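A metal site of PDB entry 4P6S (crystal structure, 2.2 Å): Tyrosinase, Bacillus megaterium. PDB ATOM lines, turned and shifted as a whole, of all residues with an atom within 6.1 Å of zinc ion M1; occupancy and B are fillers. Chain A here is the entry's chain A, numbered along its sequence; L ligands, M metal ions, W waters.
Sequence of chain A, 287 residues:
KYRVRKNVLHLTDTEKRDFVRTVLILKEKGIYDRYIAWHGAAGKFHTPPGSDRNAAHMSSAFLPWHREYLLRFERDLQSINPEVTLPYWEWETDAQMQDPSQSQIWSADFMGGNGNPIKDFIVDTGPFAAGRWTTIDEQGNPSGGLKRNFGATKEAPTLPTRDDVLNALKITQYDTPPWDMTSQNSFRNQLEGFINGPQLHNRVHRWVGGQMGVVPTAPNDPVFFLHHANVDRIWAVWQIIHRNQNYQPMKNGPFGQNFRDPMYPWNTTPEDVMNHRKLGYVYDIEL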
ATOM      1  N   HIS A  39       7.543 -22.014  19.420  1.00  0.00           N
ATOM      2  CA  HIS A  39       8.353 -22.118  18.223  1.00  0.00           C
ATOM      3  C   HIS A  39       9.316 -20.972  18.045  1.00  0.00           C
ATOM      4  O   HIS A  39      10.456 -21.185  17.718  1.00  0.00           O
ATOM      5  CB  HIS A  39       7.476 -22.321  16.990  1.00  0.00           C
ATOM      6  CG  HIS A  39       8.231 -22.345  15.711  1.00  0.00           C
ATOM      7  ND1 HIS A  39       8.408 -21.242  14.940  1.00  0.00           N
ATOM      8  CD2 HIS A  39       8.860 -23.353  15.071  1.00  0.00           C
ATOM      9  CE1 HIS A  39       9.117 -21.551  13.878  1.00  0.00           C
ATOM     10  NE2 HIS A  39       9.397 -22.832  13.938  1.00  0.00           N
ATOM     11  N   HIS A  57      15.810 -26.006  14.997  1.00  0.00           N
ATOM     12  CA  HIS A  57      16.266 -25.905  13.613  1.00  0.00           C
ATOM     13  C   HIS A  57      17.768 -26.026  13.526  1.00  0.00           C
ATOM     14  O   HIS A  57      18.455 -25.829  14.501  1.00  0.00           O
ATOM     15  CB  HIS A  57      15.890 -24.553  13.002  1.00  0.00           C
ATOM     16  CG  HIS A  57      14.447 -24.198  13.109  1.00  0.00           C
ATOM     17  ND1 HIS A  57      13.930 -23.587  14.209  1.00  0.00           N
ATOM     18  CD2 HIS A  57      13.418 -24.350  12.243  1.00  0.00           C
ATOM     19  CE1 HIS A  57      12.637 -23.396  14.034  1.00  0.00           C
ATOM     20  NE2 HIS A  57      12.310 -23.848  12.848  1.00  0.00           N
ATOM     21  N   PHE A  62      15.908 -30.926  14.916  1.00  0.00           N
ATOM     22  CA  PHE A  62      14.897 -30.383  13.994  1.00  0.00           C
ATOM     23  C   PHE A  62      13.698 -31.321  13.813  1.00  0.00           C
ATOM     24  O   PHE A  62      12.558 -30.902  13.942  1.00  0.00           O
ATOM     25  CB  PHE A  62      15.513 -30.103  12.625  1.00  0.00           C
ATOM     26  CG  PHE A  62      14.502 -29.849  11.571  1.00  0.00           C
ATOM     27  CD1 PHE A  62      13.697 -28.714  11.626  1.00  0.00           C
ATOM     28  CD2 PHE A  62      14.359 -30.728  10.499  1.00  0.00           C
ATOM     29  CE1 PHE A  62      12.743 -28.489  10.645  1.00  0.00           C
ATOM     30  CE2 PHE A  62      13.418 -30.495   9.534  1.00  0.00           C
ATOM     31  CZ  PHE A  62      12.618 -29.378   9.595  1.00  0.00           C
ATOM     32  N   HIS A  66       9.941 -31.010  15.981  1.00  0.00           N
ATOM     33  CA  HIS A  66       8.682 -30.808  15.312  1.00  0.00           C
ATOM     34  C   HIS A  66       7.664 -31.948  15.447  1.00  0.00           C
ATOM     35  O   HIS A  66       6.482 -31.677  15.511  1.00  0.00           O
ATOM     36  CB  HIS A  66       8.912 -30.426  13.856  1.00  0.00           C
ATOM     37  CG  HIS A  66       9.430 -29.041  13.663  1.00  0.00           C
ATOM     38  ND1 HIS A  66      10.764 -28.744  13.657  1.00  0.00           N
ATOM     39  CD2 HIS A  66       8.794 -27.866  13.488  1.00  0.00           C
ATOM     40  CE1 HIS A  66      10.923 -27.453  13.488  1.00  0.00           C
ATOM     41  NE2 HIS A  66       9.747 -26.893  13.377  1.00  0.00           N
ATOM     42  N   HIS A 201      12.081 -28.868   3.024  1.00  0.00           N
ATOM     43  CA  HIS A 201      11.416 -28.161   4.124  1.00  0.00           C
ATOM     44  C   HIS A 201      11.579 -26.638   4.075  1.00  0.00           C
ATOM     45  O   HIS A 201      10.590 -25.927   4.136  1.00  0.00           O
ATOM     46  CB  HIS A 201      11.850 -28.692   5.487  1.00  0.00           C
ATOM     47  CG  HIS A 201      11.595 -27.728   6.601  1.00  0.00           C
ATOM     48  ND1 HIS A 201      12.556 -26.877   7.080  1.00  0.00           N
ATOM     49  CD2 HIS A 201      10.481 -27.479   7.323  1.00  0.00           C
ATOM     50  CE1 HIS A 201      12.050 -26.143   8.055  1.00  0.00           C
ATOM     51  NE2 HIS A 201      10.791 -26.489   8.225  1.00  0.00           N
ATOM     52  N   HIS A 205       8.769 -23.359   3.037  1.00  0.00           N
ATOM     53  CA  HIS A 205       8.580 -22.136   3.808  1.00  0.00           C
ATOM     54  C   HIS A 205       8.737 -20.916   2.911  1.00  0.00           C
ATOM     55  O   HIS A 205       7.864 -20.079   2.886  1.00  0.00           O
ATOM     56  CB  HIS A 205       9.570 -22.032   4.986  1.00  0.00           C
ATOM     57  CG  HIS A 205       9.144 -22.788   6.213  1.00  0.00           C
ATOM     58  ND1 HIS A 205       8.240 -22.280   7.128  1.00  0.00           N
ATOM     59  CD2 HIS A 205       9.561 -23.984   6.712  1.00  0.00           C
ATOM     60  CE1 HIS A 205       8.082 -23.152   8.104  1.00  0.00           C
ATOM     61  NE2 HIS A 205       8.867 -24.184   7.884  1.00  0.00           N
ATOM     62  N   ALA A 218       6.486 -17.939  11.403  1.00  0.00           N
ATOM     63  CA  ALA A 218       5.939 -18.973  10.531  1.00  0.00           C
ATOM     64  C   ALA A 218       4.621 -19.631  10.974  1.00  0.00           C
ATOM     65  O   ALA A 218       3.727 -19.811  10.163  1.00  0.00           O
ATOM     66  CB  ALA A 218       6.988 -20.024  10.200  1.00  0.00           C
ATOM     67  N   PHE A 224       1.375 -24.152   8.300  1.00  0.00           N
ATOM     68  CA  PHE A 224       2.606 -24.568   8.990  1.00  0.00           C
ATOM     69  C   PHE A 224       2.458 -26.009   9.421  1.00  0.00           C
ATOM     70  O   PHE A 224       3.356 -26.829   9.215  1.00  0.00           O
ATOM     71  CB  PHE A 224       2.874 -23.691  10.240  1.00  0.00           C
ATOM     72  CG  PHE A 224       4.186 -24.027  10.990  1.00  0.00           C
ATOM     73  CD1 PHE A 224       4.225 -25.049  11.931  1.00  0.00           C
ATOM     74  CD2 PHE A 224       5.353 -23.294  10.752  1.00  0.00           C
ATOM     75  CE1 PHE A 224       5.417 -25.350  12.609  1.00  0.00           C
ATOM     76  CE2 PHE A 224       6.549 -23.601  11.443  1.00  0.00           C
ATOM     77  CZ  PHE A 224       6.565 -24.632  12.370  1.00  0.00           C
ATOM     78  N   HIS A 227       2.196 -28.484   6.490  1.00  0.00           N
ATOM     79  CA  HIS A 227       3.557 -28.633   5.944  1.00  0.00           C
ATOM     80  C   HIS A 227       4.391 -29.605   6.784  1.00  0.00           C
ATOM     81  O   HIS A 227       5.069 -30.502   6.255  1.00  0.00           O
ATOM     82  CB  HIS A 227       4.238 -27.269   5.906  1.00  0.00           C
ATOM     83  CG  HIS A 227       5.702 -27.313   5.613  1.00  0.00           C
ATOM     84  ND1 HIS A 227       6.250 -28.148   4.665  1.00  0.00           N
ATOM     85  CD2 HIS A 227       6.736 -26.629   6.159  1.00  0.00           C
ATOM     86  CE1 HIS A 227       7.557 -27.966   4.621  1.00  0.00           C
ATOM     87  NE2 HIS A 227       7.884 -27.049   5.513  1.00  0.00           N
ATOM     88  N   HIS A 228       4.348 -29.410   8.100  1.00  0.00           N
ATOM     89  CA  HIS A 228       5.196 -30.161   9.018  1.00  0.00           C
ATOM     90  C   HIS A 228       4.816 -31.646   9.171  1.00  0.00           C
ATOM     91  O   HIS A 228       5.682 -32.504   9.272  1.00  0.00           O
ATOM     92  CB  HIS A 228       5.418 -29.386  10.350  1.00  0.00           C
ATOM     93  CG  HIS A 228       6.620 -28.500  10.266  1.00  0.00           C
ATOM     94  ND1 HIS A 228       7.901 -29.020  10.359  1.00  0.00           N
ATOM     95  CD2 HIS A 228       6.762 -27.201   9.933  1.00  0.00           C
ATOM     96  CE1 HIS A 228       8.772 -28.045  10.146  1.00  0.00           C
ATOM     97  NE2 HIS A 228       8.104 -26.931   9.870  1.00  0.00           N
HETATM   98  N1  LIG L   1      15.478 -19.877   7.189  1.00  0.00           N
HETATM   99  C1  LIG L   1      15.043 -21.067   6.490  1.00  0.00           C
HETATM  100  C2  LIG L   1      15.882 -21.291   5.266  1.00  0.00           C
HETATM  101  O1  LIG L   1      15.439 -22.004   4.250  1.00  0.00           O
HETATM  102  C3  LIG L   1      13.597 -20.929   6.054  1.00  0.00           C
HETATM  103  C4  LIG L   1      12.577 -21.018   7.165  1.00  0.00           C
HETATM  104  C5  LIG L   1      11.754 -19.940   7.421  1.00  0.00           C
HETATM  105  C6  LIG L   1      12.493 -22.134   7.963  1.00  0.00           C
HETATM  106  C7  LIG L   1      10.841 -20.001   8.441  1.00  0.00           C
HETATM  107  C8  LIG L   1      11.571 -22.197   8.986  1.00  0.00           C
HETATM  108  C9  LIG L   1      10.753 -21.125   9.221  1.00  0.00           C
HETATM  109  O2  LIG L   1      11.474 -23.283   9.753  1.00  0.00           O
HETATM  110  O3  LIG L   1       9.854 -21.178  10.223  1.00  0.00           O
HETATM  111  O4  LIG L   1      16.991 -20.825   5.175  1.00  0.00           O
HETATM  112 ZN    ZN M   1       9.467 -25.534   9.556  1.00  0.00          ZN
HETATM  113 ZN    ZN M   2      10.351 -24.068  12.254  1.00  0.00          ZN
HETATM  114  O   HOH W   1       9.785 -24.790  11.062  1.00  0.00           O
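Water W1 is bound to zinc ion M1, at 1.7 Å. A ring nitrogen (NE2) of His 228 is bound to zinc ion M1 (2.0 Å). Zinc ion M1 is bound by NE2 of His 201 (2.1 Å). A ring nitrogen (NE2) of His 205 is bound to zinc ion M1 (2.2 Å).
The backbone carbonyl oxygen of His 201 sits close to a ring nitrogen (NE2) of His 227.
Residues that only touch zinc ion M1: Phe 224. Within 4 Å of zinc ion M1: His 201, His 205, Phe 224 and His 228.
Water W1 lies within hydrogen-bond range of an oxygen (O2) of the ligand and a ring nitrogen (NE2) of His 66.
NE2 of His 205 lies close to O2 of the ligand (3.3 Å). An oxygen (O2) of the ligand sits close to a ring nitrogen (NE2) of His 57, 3.3 Å away.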
